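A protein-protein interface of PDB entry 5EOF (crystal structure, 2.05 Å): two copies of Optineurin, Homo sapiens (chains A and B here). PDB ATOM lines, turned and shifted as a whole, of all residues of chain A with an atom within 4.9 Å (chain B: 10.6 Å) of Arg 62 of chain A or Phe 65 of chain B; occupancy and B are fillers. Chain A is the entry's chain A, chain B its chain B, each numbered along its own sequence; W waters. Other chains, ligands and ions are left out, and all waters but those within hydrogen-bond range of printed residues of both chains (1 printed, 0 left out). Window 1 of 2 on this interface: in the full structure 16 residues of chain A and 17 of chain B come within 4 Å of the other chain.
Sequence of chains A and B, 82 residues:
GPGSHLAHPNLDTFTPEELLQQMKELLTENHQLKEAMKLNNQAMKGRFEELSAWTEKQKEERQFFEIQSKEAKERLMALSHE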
ATOM      1  N   GLN A  58      15.791  22.652  12.349  1.00  0.00           N
ATOM      2  CA  GLN A  58      15.571  23.192  13.697  1.00  0.00           C
ATOM      3  C   GLN A  58      14.231  23.923  13.820  1.00  0.00           C
ATOM      4  O   GLN A  58      13.505  23.735  14.793  1.00  0.00           O
ATOM      5  CB  GLN A  58      16.705  24.119  14.122  1.00  0.00           C
ATOM      6  CG  GLN A  58      18.037  23.413  14.223  1.00  0.00           C
ATOM      7  CD  GLN A  58      17.993  22.279  15.202  1.00  0.00           C
ATOM      8  OE1 GLN A  58      17.757  22.488  16.387  1.00  0.00           O
ATOM      9  NE2 GLN A  58      18.212  21.060  14.716  1.00  0.00           N
ATOM     10  N   LYS A  59      13.930  24.762  12.836  1.00  0.00           N
ATOM     11  CA  LYS A  59      12.682  25.510  12.799  1.00  0.00           C
ATOM     12  C   LYS A  59      11.488  24.557  12.815  1.00  0.00           C
ATOM     13  O   LYS A  59      10.540  24.742  13.593  1.00  0.00           O
ATOM     14  CB  LYS A  59      12.647  26.391  11.546  1.00  0.00           C
ATOM     15  CG  LYS A  59      11.411  27.270  11.429  1.00  0.00           C
ATOM     16  CD  LYS A  59      11.452  28.124  10.157  1.00  0.00           C
ATOM     17  CE  LYS A  59      11.039  27.333   8.920  1.00  0.00           C
ATOM     18  NZ  LYS A  59       9.576  27.045   8.903  1.00  0.00           N
ATOM     19  N   GLU A  60      11.550  23.521  11.980  1.00  0.00           N
ATOM     20  CA  GLU A  60      10.482  22.532  11.935  1.00  0.00           C
ATOM     21  C   GLU A  60      10.303  21.806  13.265  1.00  0.00           C
ATOM     22  O   GLU A  60       9.160  21.570  13.695  1.00  0.00           O
ATOM     23  CB  GLU A  60      10.698  21.542  10.788  1.00  0.00           C
ATOM     24  CG  GLU A  60      10.581  22.197   9.405  1.00  0.00           C
ATOM     25  CD  GLU A  60      10.770  21.212   8.257  1.00  0.00           C
ATOM     26  OE1 GLU A  60      10.886  19.994   8.525  1.00  0.00           O
ATOM     27  OE2 GLU A  60      10.801  21.662   7.087  1.00  0.00           O
ATOM     28  N   GLU A  61      11.406  21.459  13.926  1.00  0.00           N
ATOM     29  CA  GLU A  61      11.291  20.800  15.226  1.00  0.00           C
ATOM     30  C   GLU A  61      10.743  21.751  16.295  1.00  0.00           C
ATOM     31  O   GLU A  61       9.858  21.371  17.082  1.00  0.00           O
ATOM     32  CB  GLU A  61      12.609  20.127  15.638  1.00  0.00           C
ATOM     33  CG  GLU A  61      12.874  18.873  14.812  1.00  0.00           C
ATOM     34  CD  GLU A  61      14.262  18.283  15.022  1.00  0.00           C
ATOM     35  OE1 GLU A  61      14.970  18.693  15.978  1.00  0.00           O
ATOM     36  OE2 GLU A  61      14.637  17.398  14.219  1.00  0.00           O
ATOM     37  N   ARG A  62      11.230  22.991  16.297  1.00  0.00           N
ATOM     38  CA  ARG A  62      10.678  24.009  17.192  1.00  0.00           C
ATOM     39  C   ARG A  62       9.163  24.126  17.027  1.00  0.00           C
ATOM     40  O   ARG A  62       8.425  24.192  18.018  1.00  0.00           O
ATOM     41  CB  ARG A  62      11.312  25.379  16.949  1.00  0.00           C
ATOM     42  CG  ARG A  62      10.643  26.478  17.760  1.00  0.00           C
ATOM     43  CD  ARG A  62      10.909  27.878  17.242  1.00  0.00           C
ATOM     44  NE  ARG A  62       9.750  28.739  17.478  1.00  0.00           N
ATOM     45  CZ  ARG A  62       9.809  30.049  17.710  1.00  0.00           C
ATOM     46  NH1 ARG A  62      10.982  30.668  17.749  1.00  0.00           N
ATOM     47  NH2 ARG A  62       8.688  30.739  17.909  1.00  0.00           N
ATOM     48  N   GLN A  63       8.699  24.145  15.782  1.00  0.00           N
ATOM     49  CA  GLN A  63       7.267  24.273  15.531  1.00  0.00           C
ATOM     50  C   GLN A  63       6.462  23.068  16.028  1.00  0.00           C
ATOM     51  O   GLN A  63       5.373  23.230  16.587  1.00  0.00           O
ATOM     52  CB  GLN A  63       6.995  24.492  14.052  1.00  0.00           C
ATOM     53  CG  GLN A  63       7.290  25.887  13.564  1.00  0.00           C
ATOM     54  CD  GLN A  63       6.751  26.114  12.162  1.00  0.00           C
ATOM     55  OE1 GLN A  63       7.469  25.941  11.170  1.00  0.00           O
ATOM     56  NE2 GLN A  63       5.473  26.487  12.073  1.00  0.00           N
ATOM     57  N   PHE A  64       6.986  21.867  15.801  1.00  0.00           N
ATOM     58  CA  PHE A  64       6.360  20.666  16.314  1.00  0.00           C
ATOM     59  C   PHE A  64       6.138  20.831  17.807  1.00  0.00           C
ATOM     60  O   PHE A  64       5.063  20.527  18.318  1.00  0.00           O
ATOM     61  CB  PHE A  64       7.212  19.423  16.047  1.00  0.00           C
ATOM     62  CG  PHE A  64       6.691  18.172  16.733  1.00  0.00           C
ATOM     63  CD1 PHE A  64       5.640  17.451  16.187  1.00  0.00           C
ATOM     64  CD2 PHE A  64       7.257  17.724  17.921  1.00  0.00           C
ATOM     65  CE1 PHE A  64       5.160  16.307  16.815  1.00  0.00           C
ATOM     66  CE2 PHE A  64       6.780  16.580  18.551  1.00  0.00           C
ATOM     67  CZ  PHE A  64       5.732  15.873  17.994  1.00  0.00           C
ATOM     68  N   PHE A  65       7.145  21.335  18.508  1.00  0.00           N
ATOM     69  CA  PHE A  65       7.039  21.440  19.961  1.00  0.00           C
ATOM     70  C   PHE A  65       6.096  22.564  20.392  1.00  0.00           C
ATOM     71  O   PHE A  65       5.353  22.390  21.361  1.00  0.00           O
ATOM     72  CB  PHE A  65       8.415  21.626  20.618  1.00  0.00           C
ATOM     73  CG  PHE A  65       9.300  20.417  20.543  1.00  0.00           C
ATOM     74  CD1 PHE A  65       8.854  19.178  20.987  1.00  0.00           C
ATOM     75  CD2 PHE A  65      10.597  20.527  20.039  1.00  0.00           C
ATOM     76  CE1 PHE A  65       9.681  18.067  20.917  1.00  0.00           C
ATOM     77  CE2 PHE A  65      11.428  19.422  19.968  1.00  0.00           C
ATOM     78  CZ  PHE A  65      10.978  18.191  20.409  1.00  0.00           C
ATOM     79  N   GLU A  66       6.128  23.712  19.704  1.00  0.00           N
ATOM     80  CA  GLU A  66       5.174  24.785  20.021  1.00  0.00           C
ATOM     81  C   GLU A  66       3.761  24.273  19.880  1.00  0.00           C
ATOM     82  O   GLU A  66       2.895  24.587  20.700  1.00  0.00           O
ATOM     83  CB  GLU A  66       5.307  25.990  19.087  1.00  0.00           C
ATOM     84  CG  GLU A  66       6.616  26.781  19.180  1.00  0.00           C
ATOM     85  CD  GLU A  66       6.542  28.109  18.419  1.00  0.00           C
ATOM     86  OE1 GLU A  66       7.308  28.294  17.444  1.00  0.00           O
ATOM     87  OE2 GLU A  66       5.709  28.963  18.795  1.00  0.00           O
ATOM     88  N   LYS B  57      21.723  29.907  19.423  1.00  0.00           N
ATOM     89  CA  LYS B  57      20.430  30.493  19.711  1.00  0.00           C
ATOM     90  C   LYS B  57      19.320  29.520  19.317  1.00  0.00           C
ATOM     91  O   LYS B  57      18.390  29.299  20.082  1.00  0.00           O
ATOM     92  CB  LYS B  57      20.260  31.830  18.992  1.00  0.00           C
ATOM     93  CG  LYS B  57      19.058  32.624  19.485  1.00  0.00           C
ATOM     94  CD  LYS B  57      18.805  33.871  18.645  1.00  0.00           C
ATOM     95  CE  LYS B  57      18.395  33.516  17.219  1.00  0.00           C
ATOM     96  NZ  LYS B  57      17.176  32.651  17.168  1.00  0.00           N
ATOM     97  N   GLN B  58      19.442  28.902  18.148  1.00  0.00           N
ATOM     98  CA  GLN B  58      18.415  27.980  17.675  1.00  0.00           C
ATOM     99  C   GLN B  58      18.304  26.695  18.485  1.00  0.00           C
ATOM    100  O   GLN B  58      17.207  26.141  18.605  1.00  0.00           O
ATOM    101  CB  GLN B  58      18.640  27.647  16.206  1.00  0.00           C
ATOM    102  CG  GLN B  58      18.799  28.885  15.358  1.00  0.00           C
ATOM    103  CD  GLN B  58      18.041  28.766  14.079  1.00  0.00           C
ATOM    104  OE1 GLN B  58      18.346  27.914  13.239  1.00  0.00           O
ATOM    105  NE2 GLN B  58      17.015  29.599  13.925  1.00  0.00           N
ATOM    106  N   LYS B  59      19.429  26.204  19.004  1.00  0.00           N
ATOM    107  CA  LYS B  59      19.410  25.046  19.907  1.00  0.00           C
ATOM    108  C   LYS B  59      18.652  25.400  21.184  1.00  0.00           C
ATOM    109  O   LYS B  59      17.759  24.658  21.615  1.00  0.00           O
ATOM    110  CB  LYS B  59      20.835  24.603  20.253  1.00  0.00           C
ATOM    111  CG  LYS B  59      21.651  24.094  19.061  1.00  0.00           C
ATOM    112  CD  LYS B  59      23.109  23.857  19.453  1.00  0.00           C
ATOM    113  CE  LYS B  59      23.914  23.234  18.323  1.00  0.00           C
ATOM    114  NZ  LYS B  59      25.316  22.962  18.744  1.00  0.00           N
ATOM    115  N   GLU B  60      19.005  26.545  21.767  1.00  0.00           N
ATOM    116  CA  GLU B  60      18.378  27.027  22.994  1.00  0.00           C
ATOM    117  C   GLU B  60      16.874  27.225  22.826  1.00  0.00           C
ATOM    118  O   GLU B  60      16.098  26.932  23.733  1.00  0.00           O
ATOM    119  CB  GLU B  60      19.044  28.329  23.455  1.00  0.00           C
ATOM    120  CG  GLU B  60      20.510  28.157  23.857  1.00  0.00           C
ATOM    121  CD  GLU B  60      21.160  29.460  24.307  1.00  0.00           C
ATOM    122  OE1 GLU B  60      20.569  30.538  24.063  1.00  0.00           O
ATOM    123  OE2 GLU B  60      22.258  29.404  24.909  1.00  0.00           O
ATOM    124  N   GLU B  61      16.464  27.709  21.658  1.00  0.00           N
ATOM    125  CA  GLU B  61      15.050  27.911  21.370  1.00  0.00           C
ATOM    126  C   GLU B  61      14.297  26.602  21.100  1.00  0.00           C
ATOM    127  O   GLU B  61      13.125  26.468  21.466  1.00  0.00           O
ATOM    128  CB  GLU B  61      14.886  28.924  20.238  1.00  0.00           C
ATOM    129  CG  GLU B  61      15.485  30.264  20.633  1.00  0.00           C
ATOM    130  CD  GLU B  61      15.210  31.375  19.644  1.00  0.00           C
ATOM    131  OE1 GLU B  61      14.571  31.100  18.599  1.00  0.00           O
ATOM    132  OE2 GLU B  61      15.634  32.524  19.927  1.00  0.00           O
ATOM    133  N   ARG B  62      14.968  25.633  20.484  1.00  0.00           N
ATOM    134  CA  ARG B  62      14.378  24.305  20.326  1.00  0.00           C
ATOM    135  C   ARG B  62      14.171  23.679  21.702  1.00  0.00           C
ATOM    136  O   ARG B  62      13.089  23.180  22.018  1.00  0.00           O
ATOM    137  CB  ARG B  62      15.276  23.394  19.486  1.00  0.00           C
ATOM    138  CG  ARG B  62      14.768  21.954  19.401  1.00  0.00           C
ATOM    139  CD  ARG B  62      15.753  21.031  18.675  1.00  0.00           C
ATOM    140  NE  ARG B  62      15.159  19.713  18.456  1.00  0.00           N
ATOM    141  CZ  ARG B  62      14.946  18.813  19.419  1.00  0.00           C
ATOM    142  NH1 ARG B  62      15.283  19.076  20.677  1.00  0.00           N
ATOM    143  NH2 ARG B  62      14.398  17.643  19.123  1.00  0.00           N
ATOM    144  N   GLN B  63      15.225  23.712  22.509  1.00  0.00           N
ATOM    145  CA  GLN B  63      15.215  23.120  23.829  1.00  0.00           C
ATOM    146  C   GLN B  63      14.163  23.755  24.739  1.00  0.00           C
ATOM    147  O   GLN B  63      13.511  23.064  25.523  1.00  0.00           O
ATOM    148  CB  GLN B  63      16.598  23.218  24.462  1.00  0.00           C
ATOM    149  CG  GLN B  63      16.676  22.557  25.818  1.00  0.00           C
ATOM    150  CD  GLN B  63      18.072  22.570  26.398  1.00  0.00           C
ATOM    151  OE1 GLN B  63      18.810  23.548  26.252  1.00  0.00           O
ATOM    152  NE2 GLN B  63      18.446  21.480  27.063  1.00  0.00           N
ATOM    153  N   PHE B  64      14.002  25.067  24.640  1.00  0.00           N
ATOM    154  CA  PHE B  64      12.967  25.738  25.411  1.00  0.00           C
ATOM    155  C   PHE B  64      11.580  25.169  25.112  1.00  0.00           C
ATOM    156  O   PHE B  64      10.794  24.880  26.035  1.00  0.00           O
ATOM    157  CB  PHE B  64      12.991  27.237  25.139  1.00  0.00           C
ATOM    158  CG  PHE B  64      11.791  27.964  25.660  1.00  0.00           C
ATOM    159  CD1 PHE B  64      11.726  28.358  26.993  1.00  0.00           C
ATOM    160  CD2 PHE B  64      10.723  28.261  24.815  1.00  0.00           C
ATOM    161  CE1 PHE B  64      10.603  29.028  27.482  1.00  0.00           C
ATOM    162  CE2 PHE B  64       9.603  28.931  25.297  1.00  0.00           C
ATOM    163  CZ  PHE B  64       9.544  29.313  26.632  1.00  0.00           C
ATOM    164  N   PHE B  65      11.259  25.011  23.831  1.00  0.00           N
ATOM    165  CA  PHE B  65       9.925  24.512  23.483  1.00  0.00           C
ATOM    166  C   PHE B  65       9.763  23.024  23.746  1.00  0.00           C
ATOM    167  O   PHE B  65       8.666  22.558  24.076  1.00  0.00           O
ATOM    168  CB  PHE B  65       9.542  24.878  22.047  1.00  0.00           C
ATOM    169  CG  PHE B  65       9.174  26.319  21.893  1.00  0.00           C
ATOM    170  CD1 PHE B  65       7.973  26.784  22.384  1.00  0.00           C
ATOM    171  CD2 PHE B  65      10.043  27.216  21.291  1.00  0.00           C
ATOM    172  CE1 PHE B  65       7.629  28.115  22.267  1.00  0.00           C
ATOM    173  CE2 PHE B  65       9.701  28.548  21.172  1.00  0.00           C
ATOM    174  CZ  PHE B  65       8.490  28.995  21.664  1.00  0.00           C
ATOM    175  N   GLU B  66      10.850  22.278  23.604  1.00  0.00           N
ATOM    176  CA  GLU B  66      10.830  20.871  23.965  1.00  0.00           C
ATOM    177  C   GLU B  66      10.510  20.694  25.448  1.00  0.00           C
ATOM    178  O   GLU B  66       9.700  19.834  25.821  1.00  0.00           O
ATOM    179  CB  GLU B  66      12.178  20.236  23.650  1.00  0.00           C
ATOM    180  CG  GLU B  66      12.252  18.755  23.956  1.00  0.00           C
ATOM    181  CD  GLU B  66      13.614  18.182  23.605  1.00  0.00           C
ATOM    182  OE1 GLU B  66      14.554  18.982  23.415  1.00  0.00           O
ATOM    183  OE2 GLU B  66      13.740  16.942  23.515  1.00  0.00           O
ATOM    184  N   ILE B  67      11.145  21.496  26.300  1.00  0.00           N
ATOM    185  CA  ILE B  67      10.876  21.406  27.737  1.00  0.00           C
ATOM    186  C   ILE B  67       9.447  21.867  28.040  1.00  0.00           C
ATOM    187  O   ILE B  67       8.730  21.246  28.841  1.00  0.00           O
ATOM    188  CB  ILE B  67      11.916  22.197  28.574  1.00  0.00           C
ATOM    189  CG1 ILE B  67      13.235  21.419  28.641  1.00  0.00           C
ATOM    190  CG2 ILE B  67      11.424  22.433  29.991  1.00  0.00           C
ATOM    191  CD1 ILE B  67      14.417  22.259  29.118  1.00  0.00           C
ATOM    192  N   GLN B  68       9.032  22.956  27.398  1.00  0.00           N
ATOM    193  CA  GLN B  68       7.671  23.454  27.561  1.00  0.00           C
ATOM    194  C   GLN B  68       6.650  22.373  27.201  1.00  0.00           C
ATOM    195  O   GLN B  68       5.726  22.111  27.957  1.00  0.00           O
ATOM    196  CB  GLN B  68       7.445  24.731  26.734  1.00  0.00           C
ATOM    197  CG  GLN B  68       6.068  25.365  26.971  1.00  0.00           C
ATOM    198  CD  GLN B  68       5.841  26.646  26.181  1.00  0.00           C
ATOM    199  OE1 GLN B  68       5.352  26.612  25.050  1.00  0.00           O
ATOM    200  NE2 GLN B  68       6.174  27.785  26.787  1.00  0.00           N
ATOM    201  N   SER B  69       6.851  21.707  26.074  1.00  0.00           N
ATOM    202  CA  SER B  69       5.929  20.670  25.625  1.00  0.00           C
ATOM    203  C   SER B  69       5.898  19.484  26.590  1.00  0.00           C
ATOM    204  O   SER B  69       4.822  18.980  26.963  1.00  0.00           O
ATOM    205  CB  SER B  69       6.317  20.199  24.219  1.00  0.00           C
ATOM    206  OG  SER B  69       5.555  19.066  23.838  1.00  0.00           O
ATOM    207  N   LYS B  70       7.083  19.043  26.993  1.00  0.00           N
ATOM    208  CA  LYS B  70       7.235  17.928  27.916  1.00  0.00           C
ATOM    209  C   LYS B  70       6.504  18.178  29.234  1.00  0.00           C
ATOM    210  O   LYS B  70       5.782  17.311  29.732  1.00  0.00           O
ATOM    211  CB  LYS B  70       8.728  17.671  28.189  1.00  0.00           C
ATOM    212  CG  LYS B  70       9.006  16.709  29.349  1.00  0.00           C
ATOM    213  CD  LYS B  70      10.471  16.757  29.784  1.00  0.00           C
ATOM    214  CE  LYS B  70      10.740  15.873  31.006  1.00  0.00           C
ATOM    215  NZ  LYS B  70      10.161  16.396  32.288  1.00  0.00           N
ATOM    216  N   GLU B  71       6.684  19.365  29.801  1.00  0.00           N
ATOM    217  CA  GLU B  71       6.075  19.671  31.086  1.00  0.00           C
ATOM    218  C   GLU B  71       4.558  19.822  30.948  1.00  0.00           C
ATOM    219  O   GLU B  71       3.810  19.445  31.843  1.00  0.00           O
ATOM    220  CB  GLU B  71       6.712  20.908  31.719  1.00  0.00           C
ATOM    221  CG  GLU B  71       8.232  20.757  31.931  1.00  0.00           C
ATOM    222  CD  GLU B  71       8.833  21.850  32.803  1.00  0.00           C
ATOM    223  OE1 GLU B  71       8.192  22.911  32.953  1.00  0.00           O
ATOM    224  OE2 GLU B  71       9.949  21.651  33.346  1.00  0.00           O
ATOM    225  N   ALA B  72       4.108  20.359  29.820  1.00  0.00           N
ATOM    226  CA  ALA B  72       2.669  20.515  29.587  1.00  0.00           C
ATOM    227  C   ALA B  72       1.965  19.164  29.501  1.00  0.00           C
ATOM    228  O   ALA B  72       0.851  18.994  30.014  1.00  0.00           O
ATOM    229  CB  ALA B  72       2.420  21.322  28.317  1.00  0.00           C
ATOM    230  N   LYS B  73       2.603  18.213  28.824  1.00  0.00           N
ATOM    231  CA  LYS B  73       2.069  16.867  28.696  1.00  0.00           C
ATOM    232  C   LYS B  73       2.060  16.166  30.049  1.00  0.00           C
ATOM    233  O   LYS B  73       1.139  15.416  30.354  1.00  0.00           O
ATOM    234  CB  LYS B  73       2.896  16.060  27.693  1.00  0.00           C
ATOM    235  CG  LYS B  73       2.741  16.511  26.234  1.00  0.00           C
ATOM    236  CD  LYS B  73       3.717  15.767  25.334  1.00  0.00           C
ATOM    237  CE  LYS B  73       3.517  16.110  23.857  1.00  0.00           C
ATOM    238  NZ  LYS B  73       2.263  15.503  23.317  1.00  0.00           N
HETATM  239  O   HOH W   1      17.404  18.277  16.464  1.00  0.00           O
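NE of Arg 62 of chain B is in salt-bridge range of OE1 of Glu 61 of chain A (2.7 Å).
The guanidinium group (NH1) of Arg 62 of chain A lies within salt-bridge range of the side-chain carboxylate (OE1) of Glu 61 of chain B (3.7 Å).
Of the 17 printed residues of chain B, 5 touch a printed residue of chain A.
Water W1 lies within hydrogen-bond range of the side-chain carboxylate of Glu 61 of chain A (2.5 Å), the guanidinium group of Arg 62 of chain B (3.3 Å) and the side-chain amide nitrogen of Gln 58 of chain A (3.4 Å).
Among the printed residues, merely in contact across the chains: Gln 58 of chain A with Arg 62 of chain B (3.4 Å), Arg 62 of chain A with Phe 65 of chain B (3.7 Å), Phe 65 of chain A with Arg 62 of chain B (3.6 Å), Phe 65 of chain A with Phe 65 of chain B (3.6 Å), Phe 65 of chain A with Glu 66 of chain B (3.8 Å), Phe 65 of chain A with Ser 69 of chain B (3.7 Å) and Glu 66 of chain A with Phe 65 of chain B (3.5 Å).
Gln 58 of chain A touches Arg 62 of chain B, but with the chains exchanged Arg 62 of chain A does not touch Gln 58 of chain B (6.2 Å).
Glu 61 of chain A touches Arg 62 of chain B, and with the chains exchanged Arg 62 of chain A touches Glu 61 of chain B.
Arg 62 of chain A touches Phe 65 of chain B, and with the chains exchanged Phe 65 of chain A touches Arg 62 of chain B.
Phe 65 of chain B touches its own counterpart, Phe 65 of chain A.
9 positions are printed for both chains.
Of the 9 pairs that touch across the chains among the printed residues, 7 have their exchanged pair printed and touching as well.
The guanidinium group (NE) of Arg 62 of chain A lies within salt-bridge range of the side-chain carboxylate (OE1) of Glu 66 of chain A.
The side-chain carboxylate (OE2) of Glu 61 of chain B is in salt-bridge range of the side-chain amino group (NZ) of Lys 57 of chain B (3.2 Å).
The side-chain carboxylate (OE1) of Glu 66 of chain B lies within salt-bridge range of the guanidinium group (NH1) of Arg 62 of chain B (2.8 Å).
Phe 64 of chain A touches none of the printed residues of chain B.
Of the printed residues of chain B, Phe 65 of chain A touches Arg 62, Phe 65, Glu 66 and Ser 69.
Of the printed residues of chain A, Arg 62 of chain B touches Gln 58 (3.4 Å), Glu 61 (2.7 Å) and Phe 65 (3.6 Å).
Of the printed residues of chain A, Ser 69 of chain B touches Phe 65.
Lys 73 of chain B touches none of the printed residues of chain A.
The nearest residue of chain B that does not touch Arg 62 of chain A is Arg 62 of chain B (4.7 Å).
The nearest printed residue of chain A that does not touch Phe 65 of chain B is Glu 61 of chain A (6.1 Å).
The nearest printed residue of chain A that does not touch Ser 69 of chain B is Glu 66 of chain A (5.7 Å).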
